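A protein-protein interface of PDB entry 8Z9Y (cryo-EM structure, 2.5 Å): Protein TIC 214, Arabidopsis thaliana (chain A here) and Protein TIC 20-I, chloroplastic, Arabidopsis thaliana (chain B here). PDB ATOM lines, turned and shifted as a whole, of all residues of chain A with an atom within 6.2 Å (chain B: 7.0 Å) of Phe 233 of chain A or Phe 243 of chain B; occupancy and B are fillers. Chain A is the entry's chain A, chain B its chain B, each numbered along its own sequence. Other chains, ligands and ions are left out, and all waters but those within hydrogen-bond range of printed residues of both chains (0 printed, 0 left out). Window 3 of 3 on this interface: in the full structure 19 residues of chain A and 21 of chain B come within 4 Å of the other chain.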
ATOM      1  N   LEU A 103       2.203  -6.780 -26.627  1.00  0.00           N
ATOM      2  CA  LEU A 103       2.792  -6.688 -25.293  1.00  0.00           C
ATOM      3  C   LEU A 103       4.205  -6.117 -25.345  1.00  0.00           C
ATOM      4  O   LEU A 103       4.557  -5.235 -24.547  1.00  0.00           O
ATOM      5  CB  LEU A 103       2.790  -8.060 -24.623  1.00  0.00           C
ATOM      6  CG  LEU A 103       1.597  -8.342 -23.708  1.00  0.00           C
ATOM      7  CD1 LEU A 103       1.299  -9.832 -23.655  1.00  0.00           C
ATOM      8  CD2 LEU A 103       1.847  -7.790 -22.315  1.00  0.00           C
ATOM      9  N   PHE A 106       4.036  -2.351 -26.197  1.00  0.00           N
ATOM     10  CA  PHE A 106       3.709  -1.584 -24.999  1.00  0.00           C
ATOM     11  C   PHE A 106       4.926  -1.432 -24.090  1.00  0.00           C
ATOM     12  O   PHE A 106       5.408  -0.312 -23.839  1.00  0.00           O
ATOM     13  CB  PHE A 106       2.558  -2.271 -24.259  1.00  0.00           C
ATOM     14  CG  PHE A 106       2.208  -1.640 -22.942  1.00  0.00           C
ATOM     15  CD1 PHE A 106       1.670  -0.366 -22.885  1.00  0.00           C
ATOM     16  CD2 PHE A 106       2.400  -2.334 -21.759  1.00  0.00           C
ATOM     17  CE1 PHE A 106       1.343   0.209 -21.671  1.00  0.00           C
ATOM     18  CE2 PHE A 106       2.074  -1.766 -20.544  1.00  0.00           C
ATOM     19  CZ  PHE A 106       1.544  -0.493 -20.500  1.00  0.00           C
ATOM     20  N   PHE A 107       5.451  -2.561 -23.604  1.00  0.00           N
ATOM     21  CA  PHE A 107       6.482  -2.528 -22.572  1.00  0.00           C
ATOM     22  C   PHE A 107       7.772  -1.866 -23.039  1.00  0.00           C
ATOM     23  O   PHE A 107       8.553  -1.410 -22.196  1.00  0.00           O
ATOM     24  CB  PHE A 107       6.776  -3.944 -22.075  1.00  0.00           C
ATOM     25  CG  PHE A 107       5.889  -4.388 -20.949  1.00  0.00           C
ATOM     26  CD1 PHE A 107       5.814  -3.653 -19.778  1.00  0.00           C
ATOM     27  CD2 PHE A 107       5.132  -5.542 -21.059  1.00  0.00           C
ATOM     28  CE1 PHE A 107       4.998  -4.058 -18.739  1.00  0.00           C
ATOM     29  CE2 PHE A 107       4.315  -5.953 -20.023  1.00  0.00           C
ATOM     30  CZ  PHE A 107       4.249  -5.210 -18.862  1.00  0.00           C
ATOM     31  N   PHE A 228      -2.592   7.489 -24.219  1.00  0.00           N
ATOM     32  CA  PHE A 228      -2.134   6.516 -25.206  1.00  0.00           C
ATOM     33  C   PHE A 228      -1.765   5.201 -24.533  1.00  0.00           C
ATOM     34  O   PHE A 228      -2.132   4.121 -25.014  1.00  0.00           O
ATOM     35  CB  PHE A 228      -0.941   7.051 -25.993  1.00  0.00           C
ATOM     36  CG  PHE A 228      -0.193   5.980 -26.735  1.00  0.00           C
ATOM     37  CD1 PHE A 228      -0.774   5.330 -27.810  1.00  0.00           C
ATOM     38  CD2 PHE A 228       1.081   5.606 -26.344  1.00  0.00           C
ATOM     39  CE1 PHE A 228      -0.096   4.338 -28.489  1.00  0.00           C
ATOM     40  CE2 PHE A 228       1.764   4.614 -27.019  1.00  0.00           C
ATOM     41  CZ  PHE A 228       1.174   3.979 -28.093  1.00  0.00           C
ATOM     42  N   SER A 229      -1.052   5.276 -23.406  1.00  0.00           N
ATOM     43  CA  SER A 229      -0.696   4.070 -22.667  1.00  0.00           C
ATOM     44  C   SER A 229      -1.934   3.358 -22.140  1.00  0.00           C
ATOM     45  O   SER A 229      -1.999   2.124 -22.150  1.00  0.00           O
ATOM     46  CB  SER A 229       0.248   4.422 -21.519  1.00  0.00           C
ATOM     47  OG  SER A 229       1.422   5.054 -22.000  1.00  0.00           O
ATOM     48  N   ILE A 230      -2.924   4.117 -21.664  1.00  0.00           N
ATOM     49  CA  ILE A 230      -4.145   3.509 -21.138  1.00  0.00           C
ATOM     50  C   ILE A 230      -4.882   2.756 -22.239  1.00  0.00           C
ATOM     51  O   ILE A 230      -5.339   1.623 -22.046  1.00  0.00           O
ATOM     52  CB  ILE A 230      -5.039   4.579 -20.489  1.00  0.00           C
ATOM     53  CG1 ILE A 230      -4.335   5.194 -19.278  1.00  0.00           C
ATOM     54  CG2 ILE A 230      -6.378   3.985 -20.085  1.00  0.00           C
ATOM     55  CD1 ILE A 230      -4.776   6.605 -18.967  1.00  0.00           C
ATOM     56  N   LEU A 231      -5.010   3.379 -23.413  1.00  0.00           N
ATOM     57  CA  LEU A 231      -5.679   2.720 -24.531  1.00  0.00           C
ATOM     58  C   LEU A 231      -4.904   1.492 -24.988  1.00  0.00           C
ATOM     59  O   LEU A 231      -5.500   0.462 -25.326  1.00  0.00           O
ATOM     60  CB  LEU A 231      -5.862   3.703 -25.687  1.00  0.00           C
ATOM     61  CG  LEU A 231      -6.850   4.844 -25.448  1.00  0.00           C
ATOM     62  CD1 LEU A 231      -6.831   5.821 -26.610  1.00  0.00           C
ATOM     63  CD2 LEU A 231      -8.251   4.300 -25.224  1.00  0.00           C
ATOM     64  N   LEU A 232      -3.571   1.581 -25.008  1.00  0.00           N
ATOM     65  CA  LEU A 232      -2.762   0.428 -25.385  1.00  0.00           C
ATOM     66  C   LEU A 232      -2.948  -0.718 -24.398  1.00  0.00           C
ATOM     67  O   LEU A 232      -3.056  -1.881 -24.799  1.00  0.00           O
ATOM     68  CB  LEU A 232      -1.292   0.836 -25.474  1.00  0.00           C
ATOM     69  CG  LEU A 232      -0.308  -0.196 -26.020  1.00  0.00           C
ATOM     70  CD1 LEU A 232      -0.874  -0.856 -27.260  1.00  0.00           C
ATOM     71  CD2 LEU A 232       1.019   0.470 -26.332  1.00  0.00           C
ATOM     72  N   PHE A 233      -2.994  -0.406 -23.102  1.00  0.00           N
ATOM     73  CA  PHE A 233      -3.213  -1.434 -22.090  1.00  0.00           C
ATOM     74  C   PHE A 233      -4.595  -2.061 -22.230  1.00  0.00           C
ATOM     75  O   PHE A 233      -4.751  -3.281 -22.087  1.00  0.00           O
ATOM     76  CB  PHE A 233      -3.029  -0.833 -20.697  1.00  0.00           C
ATOM     77  CG  PHE A 233      -3.446  -1.746 -19.583  1.00  0.00           C
ATOM     78  CD1 PHE A 233      -2.761  -2.922 -19.339  1.00  0.00           C
ATOM     79  CD2 PHE A 233      -4.523  -1.423 -18.775  1.00  0.00           C
ATOM     80  CE1 PHE A 233      -3.143  -3.761 -18.313  1.00  0.00           C
ATOM     81  CE2 PHE A 233      -4.910  -2.259 -17.748  1.00  0.00           C
ATOM     82  CZ  PHE A 233      -4.220  -3.430 -17.517  1.00  0.00           C
ATOM     83  N   ILE A 234      -5.613  -1.241 -22.501  1.00  0.00           N
ATOM     84  CA  ILE A 234      -6.963  -1.766 -22.687  1.00  0.00           C
ATOM     85  C   ILE A 234      -7.012  -2.693 -23.895  1.00  0.00           C
ATOM     86  O   ILE A 234      -7.623  -3.768 -23.848  1.00  0.00           O
ATOM     87  CB  ILE A 234      -7.973  -0.612 -22.813  1.00  0.00           C
ATOM     88  CG1 ILE A 234      -8.163   0.079 -21.464  1.00  0.00           C
ATOM     89  CG2 ILE A 234      -9.306  -1.118 -23.342  1.00  0.00           C
ATOM     90  CD1 ILE A 234      -8.721   1.478 -21.571  1.00  0.00           C
ATOM     91  N   THR A 235      -6.369  -2.293 -24.995  1.00  0.00           N
ATOM     92  CA  THR A 235      -6.324  -3.146 -26.178  1.00  0.00           C
ATOM     93  C   THR A 235      -5.583  -4.446 -25.892  1.00  0.00           C
ATOM     94  O   THR A 235      -5.990  -5.518 -26.358  1.00  0.00           O
ATOM     95  CB  THR A 235      -5.666  -2.402 -27.338  1.00  0.00           C
ATOM     96  OG1 THR A 235      -6.111  -1.041 -27.348  1.00  0.00           O
ATOM     97  CG2 THR A 235      -6.026  -3.057 -28.660  1.00  0.00           C
ATOM     98  N   CYS A 236      -4.484  -4.368 -25.138  1.00  0.00           N
ATOM     99  CA  CYS A 236      -3.739  -5.570 -24.781  1.00  0.00           C
ATOM    100  C   CYS A 236      -4.601  -6.524 -23.967  1.00  0.00           C
ATOM    101  O   CYS A 236      -4.603  -7.736 -24.208  1.00  0.00           O
ATOM    102  CB  CYS A 236      -2.476  -5.193 -24.008  1.00  0.00           C
ATOM    103  SG  CYS A 236      -1.065  -4.758 -25.046  1.00  0.00           S
ATOM    104  N   VAL A 237      -5.348  -5.990 -22.998  1.00  0.00           N
ATOM    105  CA  VAL A 237      -6.230  -6.831 -22.190  1.00  0.00           C
ATOM    106  C   VAL A 237      -7.318  -7.455 -23.056  1.00  0.00           C
ATOM    107  O   VAL A 237      -7.616  -8.651 -22.943  1.00  0.00           O
ATOM    108  CB  VAL A 237      -6.826  -6.015 -21.029  1.00  0.00           C
ATOM    109  CG1 VAL A 237      -7.998  -6.755 -20.403  1.00  0.00           C
ATOM    110  CG2 VAL A 237      -5.761  -5.723 -19.988  1.00  0.00           C
ATOM    111  N   TYR A 238      -7.923  -6.655 -23.940  1.00  0.00           N
ATOM    112  CA  TYR A 238      -8.985  -7.166 -24.800  1.00  0.00           C
ATOM    113  C   TYR A 238      -8.481  -8.294 -25.690  1.00  0.00           C
ATOM    114  O   TYR A 238      -9.155  -9.319 -25.848  1.00  0.00           O
ATOM    115  CB  TYR A 238      -9.561  -6.035 -25.650  1.00  0.00           C
ATOM    116  CG  TYR A 238     -10.955  -5.609 -25.249  1.00  0.00           C
ATOM    117  CD1 TYR A 238     -12.056  -6.399 -25.549  1.00  0.00           C
ATOM    118  CD2 TYR A 238     -11.170  -4.412 -24.578  1.00  0.00           C
ATOM    119  CE1 TYR A 238     -13.331  -6.012 -25.186  1.00  0.00           C
ATOM    120  CE2 TYR A 238     -12.443  -4.018 -24.211  1.00  0.00           C
ATOM    121  CZ  TYR A 238     -13.519  -4.822 -24.518  1.00  0.00           C
ATOM    122  OH  TYR A 238     -14.788  -4.434 -24.157  1.00  0.00           O
ATOM    123  N   LEU A 240      -5.819 -10.188 -25.066  1.00  0.00           N
ATOM    124  CA  LEU A 240      -5.505 -11.294 -24.171  1.00  0.00           C
ATOM    125  C   LEU A 240      -6.752 -12.088 -23.809  1.00  0.00           C
ATOM    126  O   LEU A 240      -6.666 -13.290 -23.536  1.00  0.00           O
ATOM    127  CB  LEU A 240      -4.804 -10.754 -22.922  1.00  0.00           C
ATOM    128  CG  LEU A 240      -4.598 -11.637 -21.694  1.00  0.00           C
ATOM    129  CD1 LEU A 240      -3.288 -11.283 -21.020  1.00  0.00           C
ATOM    130  CD2 LEU A 240      -5.744 -11.438 -20.720  1.00  0.00           C
ATOM    131  N   LEU B 136       2.991 -13.164  -7.795  1.00  0.00           N
ATOM    132  CA  LEU B 136       2.594 -13.400  -9.180  1.00  0.00           C
ATOM    133  C   LEU B 136       1.579 -14.530  -9.281  1.00  0.00           C
ATOM    134  O   LEU B 136       0.633 -14.456 -10.074  1.00  0.00           O
ATOM    135  CB  LEU B 136       3.826 -13.712 -10.028  1.00  0.00           C
ATOM    136  CG  LEU B 136       3.645 -13.762 -11.545  1.00  0.00           C
ATOM    137  CD1 LEU B 136       2.877 -12.548 -12.036  1.00  0.00           C
ATOM    138  CD2 LEU B 136       4.993 -13.867 -12.242  1.00  0.00           C
ATOM    139  N   PHE B 152      -9.613 -15.512 -19.352  1.00  0.00           N
ATOM    140  CA  PHE B 152      -8.188 -15.712 -19.105  1.00  0.00           C
ATOM    141  C   PHE B 152      -7.906 -16.058 -17.649  1.00  0.00           C
ATOM    142  O   PHE B 152      -6.877 -16.675 -17.344  1.00  0.00           O
ATOM    143  CB  PHE B 152      -7.403 -14.465 -19.510  1.00  0.00           C
ATOM    144  CG  PHE B 152      -5.962 -14.495 -19.090  1.00  0.00           C
ATOM    145  CD1 PHE B 152      -5.066 -15.350 -19.711  1.00  0.00           C
ATOM    146  CD2 PHE B 152      -5.506 -13.682 -18.067  1.00  0.00           C
ATOM    147  CE1 PHE B 152      -3.741 -15.383 -19.327  1.00  0.00           C
ATOM    148  CE2 PHE B 152      -4.181 -13.711 -17.679  1.00  0.00           C
ATOM    149  CZ  PHE B 152      -3.298 -14.564 -18.309  1.00  0.00           C
ATOM    150  N   VAL B 237      -9.332  -5.313 -10.037  1.00  0.00           N
ATOM    151  CA  VAL B 237      -8.305  -5.427  -9.004  1.00  0.00           C
ATOM    152  C   VAL B 237      -7.262  -6.466  -9.402  1.00  0.00           C
ATOM    153  O   VAL B 237      -6.052  -6.227  -9.304  1.00  0.00           O
ATOM    154  CB  VAL B 237      -8.947  -5.758  -7.644  1.00  0.00           C
ATOM    155  CG1 VAL B 237      -7.974  -6.525  -6.759  1.00  0.00           C
ATOM    156  CG2 VAL B 237      -9.400  -4.485  -6.957  1.00  0.00           C
ATOM    157  N   ALA B 238      -7.718  -7.627  -9.878  1.00  0.00           N
ATOM    158  CA  ALA B 238      -6.798  -8.698 -10.244  1.00  0.00           C
ATOM    159  C   ALA B 238      -5.903  -8.287 -11.404  1.00  0.00           C
ATOM    160  O   ALA B 238      -4.686  -8.508 -11.370  1.00  0.00           O
ATOM    161  CB  ALA B 238      -7.582  -9.964 -10.589  1.00  0.00           C
ATOM    162  N   PHE B 239      -6.486  -7.685 -12.446  1.00  0.00           N
ATOM    163  CA  PHE B 239      -5.680  -7.286 -13.596  1.00  0.00           C
ATOM    164  C   PHE B 239      -4.663  -6.217 -13.214  1.00  0.00           C
ATOM    165  O   PHE B 239      -3.489  -6.298 -13.602  1.00  0.00           O
ATOM    166  CB  PHE B 239      -6.581  -6.797 -14.728  1.00  0.00           C
ATOM    167  CG  PHE B 239      -6.984  -7.879 -15.686  1.00  0.00           C
ATOM    168  CD1 PHE B 239      -6.028  -8.574 -16.407  1.00  0.00           C
ATOM    169  CD2 PHE B 239      -8.317  -8.206 -15.864  1.00  0.00           C
ATOM    170  CE1 PHE B 239      -6.393  -9.573 -17.288  1.00  0.00           C
ATOM    171  CE2 PHE B 239      -8.688  -9.205 -16.743  1.00  0.00           C
ATOM    172  CZ  PHE B 239      -7.725  -9.889 -17.456  1.00  0.00           C
ATOM    173  N   ALA B 240      -5.091  -5.212 -12.445  1.00  0.00           N
ATOM    174  CA  ALA B 240      -4.171  -4.161 -12.030  1.00  0.00           C
ATOM    175  C   ALA B 240      -3.040  -4.723 -11.182  1.00  0.00           C
ATOM    176  O   ALA B 240      -1.876  -4.356 -11.370  1.00  0.00           O
ATOM    177  CB  ALA B 240      -4.925  -3.073 -11.265  1.00  0.00           C
ATOM    178  N   TYR B 241      -3.359  -5.624 -10.250  1.00  0.00           N
ATOM    179  CA  TYR B 241      -2.330  -6.188  -9.383  1.00  0.00           C
ATOM    180  C   TYR B 241      -1.346  -7.041 -10.178  1.00  0.00           C
ATOM    181  O   TYR B 241      -0.128  -6.954  -9.970  1.00  0.00           O
ATOM    182  CB  TYR B 241      -3.001  -6.994  -8.270  1.00  0.00           C
ATOM    183  CG  TYR B 241      -2.071  -7.765  -7.366  1.00  0.00           C
ATOM    184  CD1 TYR B 241      -1.565  -7.184  -6.212  1.00  0.00           C
ATOM    185  CD2 TYR B 241      -1.735  -9.084  -7.636  1.00  0.00           C
ATOM    186  CE1 TYR B 241      -0.729  -7.880  -5.370  1.00  0.00           C
ATOM    187  CE2 TYR B 241      -0.898  -9.791  -6.798  1.00  0.00           C
ATOM    188  CZ  TYR B 241      -0.399  -9.183  -5.666  1.00  0.00           C
ATOM    189  OH  TYR B 241       0.432  -9.880  -4.824  1.00  0.00           O
ATOM    190  N   LEU B 242      -1.855  -7.857 -11.105  1.00  0.00           N
ATOM    191  CA  LEU B 242      -0.980  -8.696 -11.916  1.00  0.00           C
ATOM    192  C   LEU B 242      -0.049  -7.855 -12.779  1.00  0.00           C
ATOM    193  O   LEU B 242       1.154  -8.136 -12.865  1.00  0.00           O
ATOM    194  CB  LEU B 242      -1.819  -9.631 -12.785  1.00  0.00           C
ATOM    195  CG  LEU B 242      -1.122 -10.256 -13.994  1.00  0.00           C
ATOM    196  CD1 LEU B 242      -0.223 -11.399 -13.563  1.00  0.00           C
ATOM    197  CD2 LEU B 242      -2.143 -10.729 -15.014  1.00  0.00           C
ATOM    198  N   PHE B 243      -0.577  -6.807 -13.415  1.00  0.00           N
ATOM    199  CA  PHE B 243       0.283  -5.985 -14.258  1.00  0.00           C
ATOM    200  C   PHE B 243       1.231  -5.127 -13.432  1.00  0.00           C
ATOM    201  O   PHE B 243       2.339  -4.826 -13.889  1.00  0.00           O
ATOM    202  CB  PHE B 243      -0.559  -5.132 -15.200  1.00  0.00           C
ATOM    203  CG  PHE B 243      -0.973  -5.856 -16.448  1.00  0.00           C
ATOM    204  CD1 PHE B 243      -0.116  -5.928 -17.533  1.00  0.00           C
ATOM    205  CD2 PHE B 243      -2.201  -6.486 -16.527  1.00  0.00           C
ATOM    206  CE1 PHE B 243      -0.485  -6.598 -18.680  1.00  0.00           C
ATOM    207  CE2 PHE B 243      -2.575  -7.159 -17.674  1.00  0.00           C
ATOM    208  CZ  PHE B 243      -1.716  -7.216 -18.751  1.00  0.00           C
ATOM    209  N   THR B 244       0.840  -4.746 -12.214  1.00  0.00           N
ATOM    210  CA  THR B 244       1.774  -4.072 -11.319  1.00  0.00           C
ATOM    211  C   THR B 244       2.943  -4.983 -10.970  1.00  0.00           C
ATOM    212  O   THR B 244       4.104  -4.553 -10.981  1.00  0.00           O
ATOM    213  CB  THR B 244       1.049  -3.618 -10.052  1.00  0.00           C
ATOM    214  OG1 THR B 244       0.171  -2.530 -10.364  1.00  0.00           O
ATOM    215  CG2 THR B 244       2.044  -3.170  -8.993  1.00  0.00           C
ATOM    216  N   VAL B 245       2.656  -6.252 -10.674  1.00  0.00           N
ATOM    217  CA  VAL B 245       3.722  -7.206 -10.376  1.00  0.00           C
ATOM    218  C   VAL B 245       4.625  -7.394 -11.591  1.00  0.00           C
ATOM    219  O   VAL B 245       5.858  -7.422 -11.472  1.00  0.00           O
ATOM    220  CB  VAL B 245       3.123  -8.539  -9.895  1.00  0.00           C
ATOM    221  CG1 VAL B 245       4.107  -9.676 -10.097  1.00  0.00           C
ATOM    222  CG2 VAL B 245       2.711  -8.437  -8.435  1.00  0.00           C
ATOM    223  N   LEU B 246       4.027  -7.519 -12.779  1.00  0.00           N
ATOM    224  CA  LEU B 246       4.824  -7.695 -13.992  1.00  0.00           C
ATOM    225  C   LEU B 246       5.710  -6.481 -14.259  1.00  0.00           C
ATOM    226  O   LEU B 246       6.875  -6.626 -14.651  1.00  0.00           O
ATOM    227  CB  LEU B 246       3.914  -7.964 -15.188  1.00  0.00           C
ATOM    228  CG  LEU B 246       3.291  -9.357 -15.264  1.00  0.00           C
ATOM    229  CD1 LEU B 246       1.902  -9.287 -15.876  1.00  0.00           C
ATOM    230  CD2 LEU B 246       4.184 -10.297 -16.058  1.00  0.00           C
ATOM    231  N   GLU B 247       5.176  -5.275 -14.060  1.00  0.00           N
ATOM    232  CA  GLU B 247       5.975  -4.078 -14.287  1.00  0.00           C
ATOM    233  C   GLU B 247       7.080  -3.944 -13.246  1.00  0.00           C
ATOM    234  O   GLU B 247       8.171  -3.459 -13.562  1.00  0.00           O
ATOM    235  CB  GLU B 247       5.076  -2.842 -14.299  1.00  0.00           C
ATOM    236  CG  GLU B 247       5.817  -1.540 -14.101  1.00  0.00           C
ATOM    237  CD  GLU B 247       6.746  -1.231 -15.252  1.00  0.00           C
ATOM    238  OE1 GLU B 247       6.384  -1.532 -16.408  1.00  0.00           O
ATOM    239  OE2 GLU B 247       7.849  -0.709 -14.997  1.00  0.00           O
ATOM    240  N   SER B 248       6.827  -4.378 -12.009  1.00  0.00           N
ATOM    241  CA  SER B 248       7.893  -4.416 -11.013  1.00  0.00           C
ATOM    242  C   SER B 248       8.994  -5.385 -11.427  1.00  0.00           C
ATOM    243  O   SER B 248      10.186  -5.102 -11.243  1.00  0.00           O
ATOM    244  CB  SER B 248       7.324  -4.799  -9.647  1.00  0.00           C
ATOM    245  OG  SER B 248       6.028  -4.258  -9.468  1.00  0.00           O
ATOM    246  N   ILE B 249       8.614  -6.538 -11.983  1.00  0.00           N
ATOM    247  CA  ILE B 249       9.609  -7.482 -12.489  1.00  0.00           C
ATOM    248  C   ILE B 249      10.423  -6.848 -13.611  1.00  0.00           C
ATOM    249  O   ILE B 249      11.650  -7.003 -13.675  1.00  0.00           O
ATOM    250  CB  ILE B 249       8.929  -8.786 -12.949  1.00  0.00           C
ATOM    251  CG1 ILE B 249       8.614  -9.679 -11.749  1.00  0.00           C
ATOM    252  CG2 ILE B 249       9.804  -9.532 -13.945  1.00  0.00           C
ATOM    253  CD1 ILE B 249       7.252 -10.326 -11.815  1.00  0.00           C
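Hydrophobic or aromatic side chains of chain A that line the printed part of chain B: Phe 107, Phe 233 and Leu 240.
Printed residues of chain B that touch a printed residue of chain A: Phe 152, Phe 239, Phe 243 and Glu 247.
Among the printed residues, no Asp or Glu carboxylate lies within 4 Å of a Lys or Arg side-chain nitrogen of the other chain.
Among the printed residues, merely in contact across the chains: Phe 107 of chain A with Glu 247 of chain B (3.7 Å), Phe 233 of chain A with Phe 243 of chain B (3.4 Å), Leu 240 of chain A with Phe 152 of chain B (3.5 Å) and Leu 240 of chain A with Phe 239 of chain B (3.96 Å).
Of chain B, only Phe 243 (3.4 Å) comes within 4 Å of Phe 233 of chain A.
Of the printed residues of chain B, Leu 240 of chain A touches Phe 152 and Phe 239.
Of the printed residues of chain A, Phe 239 of chain B touches Leu 240.
Phe 243 of chain B touches just one residue of chain A: Phe 233.
Thr 244 of chain B touches none of the printed residues of chain A.
The nearest residue of chain A that does not touch Phe 243 of chain B is Val 237 of chain A (4.2 Å).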
